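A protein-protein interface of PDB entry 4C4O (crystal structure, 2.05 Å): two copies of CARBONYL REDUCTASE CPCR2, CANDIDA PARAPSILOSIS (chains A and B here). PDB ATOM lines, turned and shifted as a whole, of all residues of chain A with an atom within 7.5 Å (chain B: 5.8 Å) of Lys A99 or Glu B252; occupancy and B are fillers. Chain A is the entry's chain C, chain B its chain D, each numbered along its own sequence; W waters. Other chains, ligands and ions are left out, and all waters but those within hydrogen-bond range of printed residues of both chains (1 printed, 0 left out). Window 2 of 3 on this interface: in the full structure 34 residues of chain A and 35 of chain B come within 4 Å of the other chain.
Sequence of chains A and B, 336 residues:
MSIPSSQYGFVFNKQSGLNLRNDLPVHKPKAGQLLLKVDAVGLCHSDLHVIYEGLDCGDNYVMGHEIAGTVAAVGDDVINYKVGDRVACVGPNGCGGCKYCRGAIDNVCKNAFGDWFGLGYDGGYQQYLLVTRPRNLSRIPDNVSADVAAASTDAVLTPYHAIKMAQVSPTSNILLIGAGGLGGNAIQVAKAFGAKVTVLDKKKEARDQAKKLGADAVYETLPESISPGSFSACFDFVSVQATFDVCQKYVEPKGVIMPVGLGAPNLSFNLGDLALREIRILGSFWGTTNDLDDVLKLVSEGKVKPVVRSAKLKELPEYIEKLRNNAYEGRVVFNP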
ATOM      1  N   CYS A  95     -19.405  18.448  24.588  1.00  0.00           N
ATOM      2  CA  CYS A  95     -18.197  18.448  23.736  1.00  0.00           C
ATOM      3  C   CYS A  95     -18.473  18.837  22.263  1.00  0.00           C
ATOM      4  O   CYS A  95     -17.612  19.398  21.597  1.00  0.00           O
ATOM      5  CB  CYS A  95     -17.492  17.097  23.809  1.00  0.00           C
ATOM      6  SG  CYS A  95     -18.252  15.779  22.831  1.00  0.00           S
ATOM      7  N   GLY A  96     -19.670  18.564  21.759  1.00  0.00           N
ATOM      8  CA  GLY A  96     -20.005  18.921  20.381  1.00  0.00           C
ATOM      9  C   GLY A  96     -19.544  17.927  19.345  1.00  0.00           C
ATOM     10  O   GLY A  96     -19.874  18.082  18.187  1.00  0.00           O
ATOM     11  N   GLY A  97     -18.794  16.895  19.751  1.00  0.00           N
ATOM     12  CA  GLY A  97     -18.211  15.952  18.800  1.00  0.00           C
ATOM     13  C   GLY A  97     -18.686  14.521  18.931  1.00  0.00           C
ATOM     14  O   GLY A  97     -18.401  13.700  18.072  1.00  0.00           O
ATOM     15  N   CYS A  98     -19.407  14.202  19.998  1.00  0.00           N
ATOM     16  CA  CYS A  98     -19.812  12.825  20.222  1.00  0.00           C
ATOM     17  C   CYS A  98     -21.212  12.592  19.656  1.00  0.00           C
ATOM     18  O   CYS A  98     -21.891  13.526  19.207  1.00  0.00           O
ATOM     19  CB  CYS A  98     -19.750  12.529  21.723  1.00  0.00           C
ATOM     20  SG  CYS A  98     -21.123  13.300  22.647  1.00  0.00           S
ATOM     21  N   LYS A  99     -21.655  11.335  19.700  1.00  0.00           N
ATOM     22  CA  LYS A  99     -22.949  10.997  19.150  1.00  0.00           C
ATOM     23  C   LYS A  99     -24.112  11.666  19.940  1.00  0.00           C
ATOM     24  O   LYS A  99     -25.163  11.942  19.359  1.00  0.00           O
ATOM     25  CB  LYS A  99     -23.160   9.481  19.065  1.00  0.00           C
ATOM     26  CG  LYS A  99     -23.241   8.755  20.396  1.00  0.00           C
ATOM     27  CD  LYS A  99     -23.476   7.277  20.106  1.00  0.00           C
ATOM     28  CE  LYS A  99     -23.684   6.460  21.378  1.00  0.00           C
ATOM     29  NZ  LYS A  99     -24.189   5.091  21.065  1.00  0.00           N
ATOM     30  N   TYR A 100     -23.928  11.871  21.256  1.00  0.00           N
ATOM     31  CA  TYR A 100     -24.979  12.484  22.094  1.00  0.00           C
ATOM     32  C   TYR A 100     -25.125  13.936  21.690  1.00  0.00           C
ATOM     33  O   TYR A 100     -26.231  14.384  21.373  1.00  0.00           O
ATOM     34  CB  TYR A 100     -24.727  12.301  23.593  1.00  0.00           C
ATOM     35  CG  TYR A 100     -24.667  10.831  23.939  1.00  0.00           C
ATOM     36  CD1 TYR A 100     -25.830  10.048  23.971  1.00  0.00           C
ATOM     37  CD2 TYR A 100     -23.436  10.198  24.145  1.00  0.00           C
ATOM     38  CE1 TYR A 100     -25.766   8.680  24.245  1.00  0.00           C
ATOM     39  CE2 TYR A 100     -23.354   8.836  24.431  1.00  0.00           C
ATOM     40  CZ  TYR A 100     -24.520   8.082  24.481  1.00  0.00           C
ATOM     41  OH  TYR A 100     -24.409   6.747  24.770  1.00  0.00           O
ATOM     42  N   CYS A 101     -24.008  14.627  21.571  1.00  0.00           N
ATOM     43  CA  CYS A 101     -24.060  16.023  21.145  1.00  0.00           C
ATOM     44  C   CYS A 101     -24.594  16.219  19.685  1.00  0.00           C
ATOM     45  O   CYS A 101     -25.215  17.232  19.394  1.00  0.00           O
ATOM     46  CB  CYS A 101     -22.682  16.651  21.314  1.00  0.00           C
ATOM     47  SG  CYS A 101     -22.184  16.898  23.030  1.00  0.00           S
ATOM     48  N   ARG A 102     -24.400  15.235  18.803  1.00  0.00           N
ATOM     49  CA  ARG A 102     -24.649  15.443  17.366  1.00  0.00           C
ATOM     50  C   ARG A 102     -26.030  15.152  16.693  1.00  0.00           C
ATOM     51  O   ARG A 102     -26.247  15.684  15.628  1.00  0.00           O
ATOM     52  CB  ARG A 102     -23.559  14.727  16.544  1.00  0.00           C
ATOM     53  CG  ARG A 102     -22.186  15.397  16.605  1.00  0.00           C
ATOM     54  CD  ARG A 102     -21.204  14.763  15.643  1.00  0.00           C
ATOM     55  NE  ARG A 102     -21.439  13.325  15.558  1.00  0.00           N
ATOM     56  CZ  ARG A 102     -20.518  12.375  15.650  1.00  0.00           C
ATOM     57  NH1 ARG A 102     -19.231  12.665  15.780  1.00  0.00           N
ATOM     58  NH2 ARG A 102     -20.902  11.112  15.542  1.00  0.00           N
ATOM     59  N   GLY A 103     -27.003  14.410  17.231  1.00  0.00           N
ATOM     60  CA  GLY A 103     -27.240  14.056  18.618  1.00  0.00           C
ATOM     61  C   GLY A 103     -28.569  14.693  19.081  1.00  0.00           C
ATOM     62  O   GLY A 103     -29.612  14.012  19.226  1.00  0.00           O
ATOM     63  N   ALA A 104     -28.516  16.010  19.291  1.00  0.00           N
ATOM     64  CA  ALA A 104     -29.580  16.824  19.943  1.00  0.00           C
ATOM     65  C   ALA A 104     -29.695  16.596  21.437  1.00  0.00           C
ATOM     66  O   ALA A 104     -30.654  17.036  22.075  1.00  0.00           O
ATOM     67  CB  ALA A 104     -30.958  16.625  19.261  1.00  0.00           C
ATOM     68  N   ILE A 105     -28.749  15.859  22.013  1.00  0.00           N
ATOM     69  CA  ILE A 105     -28.819  15.561  23.451  1.00  0.00           C
ATOM     70  C   ILE A 105     -27.493  15.882  24.097  1.00  0.00           C
ATOM     71  O   ILE A 105     -26.844  15.041  24.756  1.00  0.00           O
ATOM     72  CB  ILE A 105     -29.332  14.136  23.743  1.00  0.00           C
ATOM     73  CG1 ILE A 105     -28.529  13.081  22.984  1.00  0.00           C
ATOM     74  CG2 ILE A 105     -30.790  14.027  23.323  1.00  0.00           C
ATOM     75  CD1 ILE A 105     -29.037  11.666  23.188  1.00  0.00           C
ATOM     76  N   ASP A 106     -27.090  17.146  23.910  1.00  0.00           N
ATOM     77  CA  ASP A 106     -25.811  17.571  24.434  1.00  0.00           C
ATOM     78  C   ASP A 106     -25.803  17.664  25.963  1.00  0.00           C
ATOM     79  O   ASP A 106     -24.737  17.836  26.552  1.00  0.00           O
ATOM     80  CB  ASP A 106     -25.279  18.846  23.744  1.00  0.00           C
ATOM     81  CG  ASP A 106     -26.273  20.030  23.782  1.00  0.00           C
ATOM     82  OD1 ASP A 106     -27.242  20.047  24.571  1.00  0.00           O
ATOM     83  OD2 ASP A 106     -26.065  20.983  22.997  1.00  0.00           O
ATOM     84  N   VAL A 108     -26.408  15.180  27.923  1.00  0.00           N
ATOM     85  CA  VAL A 108     -25.897  13.910  28.477  1.00  0.00           C
ATOM     86  C   VAL A 108     -24.555  13.496  27.874  1.00  0.00           C
ATOM     87  O   VAL A 108     -24.206  12.328  27.876  1.00  0.00           O
ATOM     88  CB  VAL A 108     -26.899  12.727  28.350  1.00  0.00           C
ATOM     89  CG1 VAL A 108     -28.182  13.038  29.077  1.00  0.00           C
ATOM     90  CG2 VAL A 108     -27.179  12.354  26.899  1.00  0.00           C
ATOM     91  N   LYS A 110     -21.001  12.389  27.660  1.00  0.00           N
ATOM     92  CA  LYS A 110     -20.045  11.697  28.597  1.00  0.00           C
ATOM     93  C   LYS A 110     -18.722  12.446  28.716  1.00  0.00           C
ATOM     94  O   LYS A 110     -18.194  12.642  29.823  1.00  0.00           O
ATOM     95  CB  LYS A 110     -19.757  10.245  28.138  1.00  0.00           C
ATOM     96  CG  LYS A 110     -20.977   9.299  28.047  1.00  0.00           C
ATOM     97  CD  LYS A 110     -20.538   7.825  27.954  1.00  0.00           C
ATOM     98  CE  LYS A 110     -21.673   6.877  27.586  1.00  0.00           C
ATOM     99  NZ  LYS A 110     -21.505   5.435  28.032  1.00  0.00           N
ATOM    100  N   ASN A 111     -18.204  12.911  27.580  1.00  0.00           N
ATOM    101  CA  ASN A 111     -16.961  13.705  27.591  1.00  0.00           C
ATOM    102  C   ASN A 111     -16.967  14.974  28.473  1.00  0.00           C
ATOM    103  O   ASN A 111     -15.907  15.456  28.825  1.00  0.00           O
ATOM    104  CB  ASN A 111     -16.537  14.102  26.160  1.00  0.00           C
ATOM    105  CG  ASN A 111     -16.313  12.901  25.263  1.00  0.00           C
ATOM    106  OD1 ASN A 111     -15.941  11.836  25.737  1.00  0.00           O
ATOM    107  ND2 ASN A 111     -16.591  13.051  23.971  1.00  0.00           N
ATOM    108  N   ASN B 173     -27.889  -1.704  19.675  1.00  0.00           N
ATOM    109  CA  ASN B 173     -27.032  -2.678  20.333  1.00  0.00           C
ATOM    110  C   ASN B 173     -27.743  -3.073  21.627  1.00  0.00           C
ATOM    111  O   ASN B 173     -27.795  -2.277  22.571  1.00  0.00           O
ATOM    112  CB  ASN B 173     -25.691  -2.019  20.573  1.00  0.00           C
ATOM    113  CG  ASN B 173     -24.733  -2.931  21.341  1.00  0.00           C
ATOM    114  OD1 ASN B 173     -24.701  -4.146  21.131  1.00  0.00           O
ATOM    115  ND2 ASN B 173     -24.028  -2.349  22.269  1.00  0.00           N
ATOM    116  N   GLY B 229     -22.780   1.132  30.267  1.00  0.00           N
ATOM    117  CA  GLY B 229     -23.341   2.269  29.543  1.00  0.00           C
ATOM    118  C   GLY B 229     -23.163   2.103  28.044  1.00  0.00           C
ATOM    119  O   GLY B 229     -22.894   3.077  27.370  1.00  0.00           O
ATOM    120  N   SER B 230     -23.311   0.887  27.517  1.00  0.00           N
ATOM    121  CA  SER B 230     -23.042   0.662  26.073  1.00  0.00           C
ATOM    122  C   SER B 230     -24.192   0.071  25.241  1.00  0.00           C
ATOM    123  O   SER B 230     -24.019  -0.109  24.086  1.00  0.00           O
ATOM    124  CB  SER B 230     -21.812  -0.266  25.926  1.00  0.00           C
ATOM    125  OG  SER B 230     -22.058  -1.514  26.556  1.00  0.00           O
ATOM    126  N   PHE B 231     -25.322  -0.297  25.846  1.00  0.00           N
ATOM    127  CA  PHE B 231     -26.427  -0.883  25.141  1.00  0.00           C
ATOM    128  C   PHE B 231     -27.556   0.141  24.968  1.00  0.00           C
ATOM    129  O   PHE B 231     -27.917   0.819  25.903  1.00  0.00           O
ATOM    130  CB  PHE B 231     -26.964  -2.067  25.885  1.00  0.00           C
ATOM    131  CG  PHE B 231     -26.015  -3.243  25.893  1.00  0.00           C
ATOM    132  CD1 PHE B 231     -25.989  -4.122  24.863  1.00  0.00           C
ATOM    133  CD2 PHE B 231     -25.118  -3.404  26.913  1.00  0.00           C
ATOM    134  CE1 PHE B 231     -25.101  -5.210  24.868  1.00  0.00           C
ATOM    135  CE2 PHE B 231     -24.241  -4.488  26.951  1.00  0.00           C
ATOM    136  CZ  PHE B 231     -24.228  -5.380  25.910  1.00  0.00           C
ATOM    137  N   SER B 232     -28.113   0.226  23.763  1.00  0.00           N
ATOM    138  CA  SER B 232     -29.147   1.223  23.494  1.00  0.00           C
ATOM    139  C   SER B 232     -30.464   0.815  24.149  1.00  0.00           C
ATOM    140  O   SER B 232     -31.242   1.634  24.498  1.00  0.00           O
ATOM    141  CB  SER B 232     -29.312   1.431  21.995  1.00  0.00           C
ATOM    142  OG  SER B 232     -29.570   0.226  21.333  1.00  0.00           O
ATOM    143  N   TYR B 250     -25.685  -1.353  32.388  1.00  0.00           N
ATOM    144  CA  TYR B 250     -25.222  -1.537  31.025  1.00  0.00           C
ATOM    145  C   TYR B 250     -25.994  -0.760  29.957  1.00  0.00           C
ATOM    146  O   TYR B 250     -25.492  -0.610  28.859  1.00  0.00           O
ATOM    147  CB  TYR B 250     -25.192  -2.992  30.648  1.00  0.00           C
ATOM    148  CG  TYR B 250     -24.024  -3.654  31.327  1.00  0.00           C
ATOM    149  CD1 TYR B 250     -22.734  -3.561  30.783  1.00  0.00           C
ATOM    150  CD2 TYR B 250     -24.195  -4.325  32.539  1.00  0.00           C
ATOM    151  CE1 TYR B 250     -21.638  -4.148  31.436  1.00  0.00           C
ATOM    152  CE2 TYR B 250     -23.116  -4.934  33.190  1.00  0.00           C
ATOM    153  CZ  TYR B 250     -21.851  -4.827  32.645  1.00  0.00           C
ATOM    154  OH  TYR B 250     -20.813  -5.391  33.317  1.00  0.00           O
ATOM    155  N   VAL B 251     -27.144  -0.189  30.298  1.00  0.00           N
ATOM    156  CA  VAL B 251     -27.835   0.755  29.365  1.00  0.00           C
ATOM    157  C   VAL B 251     -27.083   2.043  29.188  1.00  0.00           C
ATOM    158  O   VAL B 251     -26.546   2.612  30.133  1.00  0.00           O
ATOM    159  CB  VAL B 251     -29.284   1.008  29.808  1.00  0.00           C
ATOM    160  CG1 VAL B 251     -29.323   1.914  31.048  1.00  0.00           C
ATOM    161  CG2 VAL B 251     -30.077   1.639  28.669  1.00  0.00           C
ATOM    162  N   GLU B 252     -26.992   2.512  27.940  1.00  0.00           N
ATOM    163  CA  GLU B 252     -26.392   3.803  27.576  1.00  0.00           C
ATOM    164  C   GLU B 252     -27.218   4.965  27.988  1.00  0.00           C
ATOM    165  O   GLU B 252     -28.427   4.858  28.098  1.00  0.00           O
ATOM    166  CB  GLU B 252     -26.489   4.044  26.020  1.00  0.00           C
ATOM    167  CG  GLU B 252     -25.593   3.304  25.121  1.00  0.00           C
ATOM    168  CD  GLU B 252     -25.967   3.498  23.670  1.00  0.00           C
ATOM    169  OE1 GLU B 252     -27.025   4.044  23.316  1.00  0.00           O
ATOM    170  OE2 GLU B 252     -25.186   3.027  22.845  1.00  0.00           O
ATOM    171  N   PRO B 253     -26.623   6.146  27.986  1.00  0.00           N
ATOM    172  CA  PRO B 253     -27.379   7.334  28.238  1.00  0.00           C
ATOM    173  C   PRO B 253     -28.504   7.483  27.203  1.00  0.00           C
ATOM    174  O   PRO B 253     -28.313   7.138  26.066  1.00  0.00           O
ATOM    175  CB  PRO B 253     -26.325   8.465  28.086  1.00  0.00           C
ATOM    176  CG  PRO B 253     -25.017   7.793  28.467  1.00  0.00           C
ATOM    177  CD  PRO B 253     -25.158   6.398  27.932  1.00  0.00           C
ATOM    178  N   LYS B 254     -29.657   7.953  27.657  1.00  0.00           N
ATOM    179  CA  LYS B 254     -30.870   8.046  26.836  1.00  0.00           C
ATOM    180  C   LYS B 254     -31.425   6.732  26.380  1.00  0.00           C
ATOM    181  O   LYS B 254     -32.362   6.685  25.577  1.00  0.00           O
ATOM    182  CB  LYS B 254     -30.644   8.930  25.612  1.00  0.00           C
ATOM    183  CG  LYS B 254     -30.976  10.343  25.868  1.00  0.00           C
ATOM    184  CD  LYS B 254     -32.478  10.483  26.154  1.00  0.00           C
ATOM    185  CE  LYS B 254     -32.958  11.874  25.730  1.00  0.00           C
ATOM    186  NZ  LYS B 254     -34.010  12.301  26.653  1.00  0.00           N
ATOM    187  N   GLY B 255     -30.890   5.646  26.885  1.00  0.00           N
ATOM    188  CA  GLY B 255     -31.332   4.344  26.460  1.00  0.00           C
ATOM    189  C   GLY B 255     -32.546   3.906  27.235  1.00  0.00           C
ATOM    190  O   GLY B 255     -33.040   4.608  28.097  1.00  0.00           O
ATOM    191  N   VAL B 256     -33.051   2.738  26.890  1.00  0.00           N
ATOM    192  CA  VAL B 256     -34.272   2.281  27.487  1.00  0.00           C
ATOM    193  C   VAL B 256     -34.095   0.923  28.195  1.00  0.00           C
ATOM    194  O   VAL B 256     -33.431   0.014  27.673  1.00  0.00           O
ATOM    195  CB  VAL B 256     -35.424   2.223  26.421  1.00  0.00           C
ATOM    196  CG1 VAL B 256     -35.059   1.350  25.260  1.00  0.00           C
ATOM    197  CG2 VAL B 256     -36.705   1.700  27.035  1.00  0.00           C
ATOM    198  N   ARG B 277     -28.294  10.425  33.366  1.00  0.00           N
ATOM    199  CA  ARG B 277     -28.074   9.842  32.072  1.00  0.00           C
ATOM    200  C   ARG B 277     -29.354   9.727  31.210  1.00  0.00           C
ATOM    201  O   ARG B 277     -29.312   9.136  30.128  1.00  0.00           O
ATOM    202  CB  ARG B 277     -27.401   8.487  32.235  1.00  0.00           C
ATOM    203  CG  ARG B 277     -26.019   8.556  32.952  1.00  0.00           C
ATOM    204  CD  ARG B 277     -25.814   7.237  33.722  1.00  0.00           C
ATOM    205  NE  ARG B 277     -25.509   6.304  32.734  1.00  0.00           N
ATOM    206  CZ  ARG B 277     -26.026   5.125  32.443  1.00  0.00           C
ATOM    207  NH1 ARG B 277     -26.864   4.418  33.155  1.00  0.00           N
ATOM    208  NH2 ARG B 277     -25.607   4.661  31.289  1.00  0.00           N
ATOM    209  N   ILE B 279     -32.178   7.959  31.536  1.00  0.00           N
ATOM    210  CA  ILE B 279     -32.635   6.611  31.238  1.00  0.00           C
ATOM    211  C   ILE B 279     -34.162   6.608  31.267  1.00  0.00           C
ATOM    212  O   ILE B 279     -34.756   7.331  32.014  1.00  0.00           O
ATOM    213  CB  ILE B 279     -32.084   5.589  32.282  1.00  0.00           C
ATOM    214  CG1 ILE B 279     -30.567   5.712  32.401  1.00  0.00           C
ATOM    215  CG2 ILE B 279     -32.444   4.168  31.913  1.00  0.00           C
ATOM    216  CD1 ILE B 279     -29.831   5.629  31.100  1.00  0.00           C
HETATM  217  O   HOH W   1     -27.246   4.201  20.477  1.00  0.00           O
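The side-chain amino group of Lys A99 is in salt-bridge range of the side-chain carboxylate of Glu B252 (2.9 Å).
NZ of Lys A110 is in hydrogen-bond range of O of Gly B229.
The backbone NH of Tyr A100 sits close to the side-chain sulfur of Cys A98 (3.4 Å).
The backbone NH (N) of Ile A105 lies within hydrogen-bond range of the backbone carbonyl oxygen (O) of Tyr A100 (3.0 Å).
The backbone carbonyl oxygen (O) of Phe B231 sits at hydrogen-bond distance from the backbone NH (N) of Glu B252, at 2.8 Å.
N of Lys B254 lies within hydrogen-bond range of O of Arg B277.
Tyr A100 touches Glu B252 (OH to CB, 3.6 Å).
Tyr A100 touches Pro B253 (OH to CD, 3.3 Å).
Lys B254 touches Ile A105.
CE of Lys A110 touches CD of Pro B253, at 3.5 Å.
Printed residues of chain B within 4 Å of Lys A99: Glu B252 (2.9 Å).
Of the printed residues of chain B, Ile A105 touches Lys B254.
Of the printed residues of chain B, Lys A110 touches Gly B229 (2.8 Å) and Pro B253 (3.5 Å).
Printed residues of chain A within 4 Å of Gly B229: Lys A110.
Glu B252 touches two residues of chain A.
The nearest printed residue of chain B that does not touch Lys A99 is Ser B230 (6.0 Å).
The nearest printed residue of chain B that does not touch Tyr A100 is Gly B229 (4.7 Å).
Of the 14 printed residues of chain B, 4 touch a printed residue of chain A.
Hydrophobic or aromatic side chains of chain B that line the printed part of chain A: Pro B253.
Along chain B the printed residues that touch a printed residue of chain A span positions 229 to 254.
Of the 15 printed residues of chain A, 4 touch a printed residue of chain B.
Hydrophobic or aromatic side chains of chain A within 4 Å of the printed part of chain B: Tyr A100 and Ile A105.
Among the printed residues, 6 pairs touch across the chains.
No position is printed for both chains.
Of the 6 pairs that touch across the chains among the printed residues, none has its exchanged pair printed and touching as well.
Water W1 bridges OE1 of Glu B252 (2.9 Å) and NZ of Lys A99 (3.2 Å).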
